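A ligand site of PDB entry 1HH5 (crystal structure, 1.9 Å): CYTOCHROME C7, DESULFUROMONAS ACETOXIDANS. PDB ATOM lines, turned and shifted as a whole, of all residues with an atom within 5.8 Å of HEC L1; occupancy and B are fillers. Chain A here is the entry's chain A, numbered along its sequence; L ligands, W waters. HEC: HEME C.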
ATOM      1  N   ALA A   1      33.302 -21.972  31.437  1.00  0.00           N
ATOM      2  CA  ALA A   1      34.727 -22.023  30.990  1.00  0.00           C
ATOM      3  C   ALA A   1      35.227 -20.621  30.700  1.00  0.00           C
ATOM      4  O   ALA A   1      34.455 -19.659  30.699  1.00  0.00           O
ATOM      5  CB  ALA A   1      34.868 -22.887  29.749  1.00  0.00           C
ATOM      6  N   VAL A   4      34.897 -20.010  25.033  1.00  0.00           N
ATOM      7  CA  VAL A   4      33.834 -20.797  24.432  1.00  0.00           C
ATOM      8  C   VAL A   4      33.839 -20.592  22.930  1.00  0.00           C
ATOM      9  O   VAL A   4      33.936 -19.467  22.449  1.00  0.00           O
ATOM     10  CB  VAL A   4      32.445 -20.354  24.958  1.00  0.00           C
ATOM     11  CG1 VAL A   4      31.353 -21.177  24.302  1.00  0.00           C
ATOM     12  CG2 VAL A   4      32.397 -20.502  26.470  1.00  0.00           C
ATOM     13  N   TYR A   6      31.788 -21.312  19.319  1.00  0.00           N
ATOM     14  CA  TYR A   6      30.513 -21.664  18.728  1.00  0.00           C
ATOM     15  C   TYR A   6      30.775 -22.055  17.283  1.00  0.00           C
ATOM     16  O   TYR A   6      30.872 -21.199  16.398  1.00  0.00           O
ATOM     17  CB  TYR A   6      29.547 -20.479  18.798  1.00  0.00           C
ATOM     18  CG  TYR A   6      29.329 -19.951  20.194  1.00  0.00           C
ATOM     19  CD1 TYR A   6      28.416 -20.558  21.052  1.00  0.00           C
ATOM     20  CD2 TYR A   6      30.026 -18.843  20.675  1.00  0.00           C
ATOM     21  CE1 TYR A   6      28.202 -20.087  22.345  1.00  0.00           C
ATOM     22  CE2 TYR A   6      29.817 -18.359  21.966  1.00  0.00           C
ATOM     23  CZ  TYR A   6      28.896 -18.983  22.793  1.00  0.00           C
ATOM     24  OH  TYR A   6      28.670 -18.503  24.068  1.00  0.00           O
ATOM     25  N   PHE A  15      34.386 -17.027  21.829  1.00  0.00           N
ATOM     26  CA  PHE A  15      33.960 -16.137  22.894  1.00  0.00           C
ATOM     27  C   PHE A  15      34.882 -16.298  24.094  1.00  0.00           C
ATOM     28  O   PHE A  15      34.795 -17.276  24.833  1.00  0.00           O
ATOM     29  CB  PHE A  15      32.527 -16.442  23.316  1.00  0.00           C
ATOM     30  CG  PHE A  15      32.044 -15.619  24.492  1.00  0.00           C
ATOM     31  CD1 PHE A  15      32.275 -14.252  24.548  1.00  0.00           C
ATOM     32  CD2 PHE A  15      31.336 -16.226  25.523  1.00  0.00           C
ATOM     33  CE1 PHE A  15      31.791 -13.494  25.611  1.00  0.00           C
ATOM     34  CE2 PHE A  15      30.846 -15.481  26.588  1.00  0.00           C
ATOM     35  CZ  PHE A  15      31.089 -14.112  26.636  1.00  0.00           C
ATOM     36  N   HIS A  17      35.314 -15.693  27.327  1.00  0.00           N
ATOM     37  CA  HIS A  17      34.529 -15.355  28.512  1.00  0.00           C
ATOM     38  C   HIS A  17      35.359 -14.652  29.576  1.00  0.00           C
ATOM     39  O   HIS A  17      34.912 -13.663  30.160  1.00  0.00           O
ATOM     40  CB  HIS A  17      33.927 -16.640  29.072  1.00  0.00           C
ATOM     41  CG  HIS A  17      32.983 -16.422  30.216  1.00  0.00           C
ATOM     42  ND1 HIS A  17      33.274 -16.710  31.528  1.00  0.00           N
ATOM     43  CD2 HIS A  17      31.716 -15.944  30.221  1.00  0.00           C
ATOM     44  CE1 HIS A  17      32.196 -16.426  32.270  1.00  0.00           C
ATOM     45  NE2 HIS A  17      31.220 -15.959  31.531  1.00  0.00           N
ATOM     46  N   HIS A  20      36.257 -10.944  28.523  1.00  0.00           N
ATOM     47  CA  HIS A  20      35.094 -10.071  28.654  1.00  0.00           C
ATOM     48  C   HIS A  20      34.846  -9.741  30.134  1.00  0.00           C
ATOM     49  O   HIS A  20      34.589  -8.589  30.491  1.00  0.00           O
ATOM     50  CB  HIS A  20      33.839 -10.737  28.079  1.00  0.00           C
ATOM     51  CG  HIS A  20      33.725 -10.614  26.582  1.00  0.00           C
ATOM     52  ND1 HIS A  20      34.492 -11.321  25.683  1.00  0.00           N
ATOM     53  CD2 HIS A  20      32.889  -9.856  25.836  1.00  0.00           C
ATOM     54  CE1 HIS A  20      34.097 -10.971  24.447  1.00  0.00           C
ATOM     55  NE2 HIS A  20      33.124 -10.081  24.496  1.00  0.00           N
ATOM     56  N   ALA A  21      34.912 -10.753  30.993  1.00  0.00           N
ATOM     57  CA  ALA A  21      34.683 -10.556  32.421  1.00  0.00           C
ATOM     58  C   ALA A  21      35.675  -9.590  33.041  1.00  0.00           C
ATOM     59  O   ALA A  21      35.307  -8.768  33.882  1.00  0.00           O
ATOM     60  CB  ALA A  21      34.740 -11.903  33.149  1.00  0.00           C
ATOM     61  N   LEU A  24      34.616  -6.003  31.722  1.00  0.00           N
ATOM     62  CA  LEU A  24      33.283  -5.523  32.046  1.00  0.00           C
ATOM     63  C   LEU A  24      32.754  -5.836  33.427  1.00  0.00           C
ATOM     64  O   LEU A  24      31.993  -5.055  33.995  1.00  0.00           O
ATOM     65  CB  LEU A  24      32.306  -6.056  30.998  1.00  0.00           C
ATOM     66  CG  LEU A  24      32.679  -5.704  29.561  1.00  0.00           C
ATOM     67  CD1 LEU A  24      32.068  -6.703  28.601  1.00  0.00           C
ATOM     68  CD2 LEU A  24      32.214  -4.282  29.262  1.00  0.00           C
ATOM     69  N   GLY A  25      33.138  -6.992  33.968  1.00  0.00           N
ATOM     70  CA  GLY A  25      32.629  -7.381  35.268  1.00  0.00           C
ATOM     71  C   GLY A  25      31.398  -8.220  35.010  1.00  0.00           C
ATOM     72  O   GLY A  25      30.721  -8.035  34.001  1.00  0.00           O
ATOM     73  N   CYS A  26      31.097  -9.119  35.935  1.00  0.00           N
ATOM     74  CA  CYS A  26      29.976 -10.051  35.811  1.00  0.00           C
ATOM     75  C   CYS A  26      28.590  -9.484  35.503  1.00  0.00           C
ATOM     76  O   CYS A  26      27.910  -9.989  34.608  1.00  0.00           O
ATOM     77  CB  CYS A  26      29.910 -10.919  37.076  1.00  0.00           C
ATOM     78  SG  CYS A  26      31.488 -11.719  37.471  1.00  0.00           S
ATOM     79  N   ALA A  28      27.657  -7.109  33.887  1.00  0.00           N
ATOM     80  CA  ALA A  28      27.524  -6.448  32.604  1.00  0.00           C
ATOM     81  C   ALA A  28      26.604  -7.333  31.763  1.00  0.00           C
ATOM     82  O   ALA A  28      25.854  -6.843  30.921  1.00  0.00           O
ATOM     83  CB  ALA A  28      28.879  -6.315  31.931  1.00  0.00           C
ATOM     84  N   CYS A  29      26.649  -8.646  32.011  1.00  0.00           N
ATOM     85  CA  CYS A  29      25.835  -9.592  31.249  1.00  0.00           C
ATOM     86  C   CYS A  29      24.981 -10.529  32.076  1.00  0.00           C
ATOM     87  O   CYS A  29      24.019 -11.102  31.566  1.00  0.00           O
ATOM     88  CB  CYS A  29      26.735 -10.458  30.369  1.00  0.00           C
ATOM     89  SG  CYS A  29      28.056  -9.547  29.552  1.00  0.00           S
ATOM     90  N   HIS A  30      25.350 -10.702  33.336  1.00  0.00           N
ATOM     91  CA  HIS A  30      24.618 -11.610  34.219  1.00  0.00           C
ATOM     92  C   HIS A  30      23.807 -10.875  35.271  1.00  0.00           C
ATOM     93  O   HIS A  30      24.321 -10.016  35.986  1.00  0.00           O
ATOM     94  CB  HIS A  30      25.604 -12.541  34.940  1.00  0.00           C
ATOM     95  CG  HIS A  30      26.230 -13.559  34.053  1.00  0.00           C
ATOM     96  ND1 HIS A  30      25.565 -14.649  33.534  1.00  0.00           N
ATOM     97  CD2 HIS A  30      27.498 -13.650  33.585  1.00  0.00           C
ATOM     98  CE1 HIS A  30      26.437 -15.357  32.794  1.00  0.00           C
ATOM     99  NE2 HIS A  30      27.625 -14.782  32.798  1.00  0.00           N
ATOM    100  N   PRO A  34      25.295 -15.530  38.615  1.00  0.00           N
ATOM    101  CA  PRO A  34      25.743 -15.880  37.269  1.00  0.00           C
ATOM    102  C   PRO A  34      25.361 -17.305  36.867  1.00  0.00           C
ATOM    103  O   PRO A  34      25.681 -18.262  37.567  1.00  0.00           O
ATOM    104  CB  PRO A  34      27.260 -15.695  37.357  1.00  0.00           C
ATOM    105  CG  PRO A  34      27.383 -14.566  38.323  1.00  0.00           C
ATOM    106  CD  PRO A  34      26.407 -14.956  39.400  1.00  0.00           C
ATOM    107  N   ALA A  35      24.680 -17.423  35.740  1.00  0.00           N
ATOM    108  CA  ALA A  35      24.254 -18.717  35.226  1.00  0.00           C
ATOM    109  C   ALA A  35      24.438 -18.725  33.711  1.00  0.00           C
ATOM    110  O   ALA A  35      24.686 -17.691  33.102  1.00  0.00           O
ATOM    111  CB  ALA A  35      22.793 -18.961  35.574  1.00  0.00           C
ATOM    112  N   LYS A  36      24.310 -19.905  33.125  1.00  0.00           N
ATOM    113  CA  LYS A  36      24.467 -20.069  31.682  1.00  0.00           C
ATOM    114  C   LYS A  36      23.501 -19.161  30.920  1.00  0.00           C
ATOM    115  O   LYS A  36      22.360 -18.960  31.334  1.00  0.00           O
ATOM    116  CB  LYS A  36      24.226 -21.526  31.285  1.00  0.00           C
ATOM    117  CG  LYS A  36      24.692 -21.864  29.875  1.00  0.00           C
ATOM    118  CD  LYS A  36      24.450 -23.326  29.546  1.00  0.00           C
ATOM    119  CE  LYS A  36      25.158 -23.712  28.248  1.00  0.00           C
ATOM    120  NZ  LYS A  36      26.640 -23.659  28.387  1.00  0.00           N
ATOM    121  N   ILE A  37      23.981 -18.612  29.815  1.00  0.00           N
ATOM    122  CA  ILE A  37      23.165 -17.741  28.963  1.00  0.00           C
ATOM    123  C   ILE A  37      23.047 -18.457  27.616  1.00  0.00           C
ATOM    124  O   ILE A  37      24.050 -18.688  26.951  1.00  0.00           O
ATOM    125  CB  ILE A  37      23.835 -16.367  28.743  1.00  0.00           C
ATOM    126  CG1 ILE A  37      23.868 -15.583  30.060  1.00  0.00           C
ATOM    127  CG2 ILE A  37      23.071 -15.583  27.682  1.00  0.00           C
ATOM    128  CD1 ILE A  37      24.543 -14.211  29.931  1.00  0.00           C
ATOM    129  N   ALA A  38      21.822 -18.786  27.234  1.00  0.00           N
ATOM    130  CA  ALA A  38      21.566 -19.492  25.978  1.00  0.00           C
ATOM    131  C   ALA A  38      21.961 -18.629  24.789  1.00  0.00           C
ATOM    132  O   ALA A  38      21.431 -17.544  24.582  1.00  0.00           O
ATOM    133  CB  ALA A  38      20.085 -19.855  25.881  1.00  0.00           C
ATOM    134  N   ILE A  39      22.908 -19.129  24.000  1.00  0.00           N
ATOM    135  CA  ILE A  39      23.369 -18.405  22.833  1.00  0.00           C
ATOM    136  C   ILE A  39      22.986 -19.083  21.523  1.00  0.00           C
ATOM    137  O   ILE A  39      23.361 -20.226  21.282  1.00  0.00           O
ATOM    138  CB  ILE A  39      24.911 -18.236  22.836  1.00  0.00           C
ATOM    139  CG1 ILE A  39      25.349 -17.397  24.038  1.00  0.00           C
ATOM    140  CG2 ILE A  39      25.362 -17.575  21.541  1.00  0.00           C
ATOM    141  CD1 ILE A  39      24.756 -15.991  24.074  1.00  0.00           C
ATOM    142  N   ALA A  48      22.497 -10.561  23.290  1.00  0.00           N
ATOM    143  CA  ALA A  48      23.498 -11.390  23.962  1.00  0.00           C
ATOM    144  C   ALA A  48      24.942 -11.059  23.536  1.00  0.00           C
ATOM    145  O   ALA A  48      25.867 -11.244  24.324  1.00  0.00           O
ATOM    146  CB  ALA A  48      23.206 -12.879  23.723  1.00  0.00           C
HETATM  147 FE   HEC L   1      29.437 -15.366  32.224  1.00  0.00          FE
HETATM  148  CHA HEC L   1      28.149 -18.374  31.136  1.00  0.00           C
HETATM  149  CHB HEC L   1      29.968 -16.729  35.329  1.00  0.00           C
HETATM  150  CHC HEC L   1      31.080 -12.522  33.201  1.00  0.00           C
HETATM  151  CHD HEC L   1      28.521 -13.907  29.316  1.00  0.00           C
HETATM  152  NA  HEC L   1      29.100 -17.140  33.042  1.00  0.00           N
HETATM  153  C1A HEC L   1      28.531 -18.263  32.468  1.00  0.00           C
HETATM  154  C2A HEC L   1      28.333 -19.318  33.445  1.00  0.00           C
HETATM  155  C3A HEC L   1      28.845 -18.862  34.616  1.00  0.00           C
HETATM  156  C4A HEC L   1      29.345 -17.523  34.367  1.00  0.00           C
HETATM  157  CMA HEC L   1      28.856 -19.600  35.967  1.00  0.00           C
HETATM  158  CAA HEC L   1      27.537 -20.611  33.240  1.00  0.00           C
HETATM  159  CBA HEC L   1      28.146 -21.927  33.691  1.00  0.00           C
HETATM  160  CGA HEC L   1      29.279 -22.395  32.804  1.00  0.00           C
HETATM  161  O1A HEC L   1      30.283 -21.669  32.662  1.00  0.00           O
HETATM  162  O2A HEC L   1      29.159 -23.513  32.245  1.00  0.00           O
HETATM  163  NB  HEC L   1      30.303 -14.748  33.892  1.00  0.00           N
HETATM  164  C1B HEC L   1      30.401 -15.433  35.126  1.00  0.00           C
HETATM  165  C2B HEC L   1      31.116 -14.668  36.096  1.00  0.00           C
HETATM  166  C3B HEC L   1      31.534 -13.535  35.473  1.00  0.00           C
HETATM  167  C4B HEC L   1      30.987 -13.560  34.122  1.00  0.00           C
HETATM  168  CMB HEC L   1      31.267 -14.999  37.593  1.00  0.00           C
HETATM  169  CAB HEC L   1      32.429 -12.463  36.081  1.00  0.00           C
HETATM  170  CBB HEC L   1      33.835 -12.959  36.396  1.00  0.00           C
HETATM  171  NC  HEC L   1      29.689 -13.574  31.446  1.00  0.00           N
HETATM  172  C1C HEC L   1      30.431 -12.519  31.949  1.00  0.00           C
HETATM  173  C2C HEC L   1      30.361 -11.377  31.070  1.00  0.00           C
HETATM  174  C3C HEC L   1      29.540 -11.748  30.028  1.00  0.00           C
HETATM  175  C4C HEC L   1      29.179 -13.124  30.249  1.00  0.00           C
HETATM  176  CMC HEC L   1      31.032 -10.023  31.289  1.00  0.00           C
HETATM  177  CAC HEC L   1      29.075 -10.897  28.844  1.00  0.00           C
HETATM  178  CBC HEC L   1      30.219 -10.455  27.932  1.00  0.00           C
HETATM  179  ND  HEC L   1      28.577 -16.024  30.570  1.00  0.00           N
HETATM  180  C1D HEC L   1      28.254 -15.275  29.446  1.00  0.00           C
HETATM  181  C2D HEC L   1      27.667 -16.111  28.410  1.00  0.00           C
HETATM  182  C3D HEC L   1      27.595 -17.359  28.906  1.00  0.00           C
HETATM  183  C4D HEC L   1      28.152 -17.309  30.253  1.00  0.00           C
HETATM  184  CMD HEC L   1      27.263 -15.700  27.008  1.00  0.00           C
HETATM  185  CAD HEC L   1      27.165 -18.609  28.133  1.00  0.00           C
HETATM  186  CBD HEC L   1      28.406 -19.302  27.554  1.00  0.00           C
HETATM  187  CGD HEC L   1      28.066 -20.589  26.825  1.00  0.00           C
HETATM  188  O1D HEC L   1      27.606 -20.524  25.666  1.00  0.00           O
HETATM  189  O2D HEC L   1      28.245 -21.658  27.433  1.00  0.00           O
HETATM  190 FE   HEC L   2      32.279  -9.114  22.984  1.00  0.00          FE
HETATM  191  CHA HEC L   2      35.331  -7.950  21.979  1.00  0.00           C
HETATM  192  CHB HEC L   2      32.686 -11.896  20.940  1.00  0.00           C
HETATM  193  CHC HEC L   2      29.287 -10.326  24.037  1.00  0.00           C
HETATM  194  CHD HEC L   2      31.837  -6.341  24.941  1.00  0.00           C
HETATM  195  NA  HEC L   2      33.679  -9.771  21.754  1.00  0.00           N
HETATM  196  C1A HEC L   2      34.875  -9.146  21.424  1.00  0.00           C
HETATM  197  C2A HEC L   2      35.548  -9.873  20.363  1.00  0.00           C
HETATM  198  C3A HEC L   2      34.818 -10.969  20.066  1.00  0.00           C
HETATM  199  C4A HEC L   2      33.679 -10.938  20.954  1.00  0.00           C
HETATM  200  CMA HEC L   2      35.083 -12.000  18.966  1.00  0.00           C
HETATM  201  CAA HEC L   2      36.747  -9.356  19.614  1.00  0.00           C
HETATM  202  CBA HEC L   2      38.090 -10.010  19.901  1.00  0.00           C
HETATM  203  CGA HEC L   2      38.421 -10.079  21.370  1.00  0.00           C
HETATM  204  O1A HEC L   2      38.075 -11.091  22.014  1.00  0.00           O
HETATM  205  O2A HEC L   2      39.021  -9.104  21.879  1.00  0.00           O
HETATM  206  NB  HEC L   2      31.235 -10.735  22.571  1.00  0.00           N
HETATM  207  C1B HEC L   2      31.521 -11.790  21.707  1.00  0.00           C
HETATM  208  C2B HEC L   2      30.473 -12.783  21.717  1.00  0.00           C
HETATM  209  C3B HEC L   2      29.565 -12.386  22.630  1.00  0.00           C
HETATM  210  C4B HEC L   2      30.031 -11.101  23.139  1.00  0.00           C
HETATM  211  CMB HEC L   2      30.344 -13.940  20.747  1.00  0.00           C
HETATM  212  CAB HEC L   2      28.279 -13.080  23.071  1.00  0.00           C
HETATM  213  CBB HEC L   2      28.484 -14.512  23.557  1.00  0.00           C
HETATM  214  NC  HEC L   2      30.815  -8.442  24.154  1.00  0.00           N
HETATM  215  C1C HEC L   2      29.639  -9.055  24.465  1.00  0.00           C
HETATM  216  C2C HEC L   2      28.838  -8.228  25.349  1.00  0.00           C
HETATM  217  C3C HEC L   2      29.541  -7.088  25.611  1.00  0.00           C
HETATM  218  C4C HEC L   2      30.777  -7.234  24.871  1.00  0.00           C
HETATM  219  CMC HEC L   2      27.446  -8.571  25.830  1.00  0.00           C
HETATM  220  CAC HEC L   2      29.196  -5.866  26.458  1.00  0.00           C
HETATM  221  CBC HEC L   2      28.160  -6.017  27.572  1.00  0.00           C
HETATM  222  ND  HEC L   2      33.331  -7.529  23.389  1.00  0.00           N
HETATM  223  C1D HEC L   2      33.047  -6.516  24.289  1.00  0.00           C
HETATM  224  C2D HEC L   2      34.175  -5.607  24.433  1.00  0.00           C
HETATM  225  C3D HEC L   2      35.068  -5.991  23.511  1.00  0.00           C
HETATM  226  C4D HEC L   2      34.595  -7.198  22.898  1.00  0.00           C
HETATM  227  CMD HEC L   2      34.380  -4.447  25.419  1.00  0.00           C
HETATM  228  CAD HEC L   2      36.224  -5.105  23.119  1.00  0.00           C
HETATM  229  CBD HEC L   2      37.569  -5.514  23.629  1.00  0.00           C
HETATM  230  CGD HEC L   2      38.534  -4.349  23.658  1.00  0.00           C
HETATM  231  O1D HEC L   2      38.524  -3.545  22.706  1.00  0.00           O
HETATM  232  O2D HEC L   2      39.305  -4.238  24.641  1.00  0.00           O
HETATM  233  O   HOH W   1      29.503 -23.913  27.534  1.00  0.00           O
HETATM  234  O   HOH W   2      32.456 -19.875  33.537  1.00  0.00           O
HETATM  235  O   HOH W   3      35.238 -15.215  34.701  1.00  0.00           O
HETATM  236  O   HOH W   4      25.030 -21.087  25.736  1.00  0.00           O
HETATM  237  O   HOH W   5      27.955 -23.378  25.052  1.00  0.00           O
HETATM  238  O   HOH W   6      31.384 -19.310  30.485  1.00  0.00           O
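The side-chain hydroxyl of Tyr 6 is in hydrogen-bond range of an oxygen (O1D) of HEC L1 (2.8 Å).
CAB of HEC L1 is bonded to SG of Cys 26, at 1.8 Å.
A ring nitrogen (NE2) of His 30 is bound to an iron atom (FE) of HEC L1 (2.0 Å).
NZ of Lys 36 is in salt-bridge range of O2D of HEC L1 (2.7 Å).
N of Ala 1 sits at hydrogen-bond distance from O1A of HEC L1.
An iron atom (FE) of HEC L1 is bound by a ring nitrogen (NE2) of His 17 (2.0 Å).
NE2 of His 20 is bound to FE of HEC L2.
A carbon (CAC) of HEC L1 is covalently linked to the side-chain sulfur (SG) of Cys 29 (1.8 Å).
Residues that only touch HEC L1: Ile 37, Gly 25, His 20, Ala 21, Pro 34, Phe 15, Ala 35 and Ile 39.
The nearest printed residue that does not touch HEC L1 is Val 4 (4.04 Å).
Water W1 lies within hydrogen-bond range of O2D of HEC L1 (2.6 Å) and NZ of Lys 36 (3.0 Å).
Water W4 lies within hydrogen-bond range of an oxygen (O1D) of HEC L1, the backbone carbonyl oxygen of Ile 37 and the backbone NH of Ile 39.
Water W2 lies within hydrogen-bond range of an oxygen (O1A) of HEC L1 (3.0 Å) and the backbone NH (N) of Ala 1 (3.1 Å).
Water W6 lies within hydrogen-bond range of the backbone carbonyl oxygen of Ala 1, a ring nitrogen (ND1) of His 17 and an oxygen (O1A) of HEC L1.
ND1 of His 17 lies within hydrogen-bond range of O of Ala 1 (3.3 Å).
O of Ala 35 sits close to ND1 of His 30, at 3.2 Å.
The backbone carbonyl oxygen (O) of Val 4 sits at hydrogen-bond distance from the backbone NH (N) of Phe 15 (2.6 Å).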
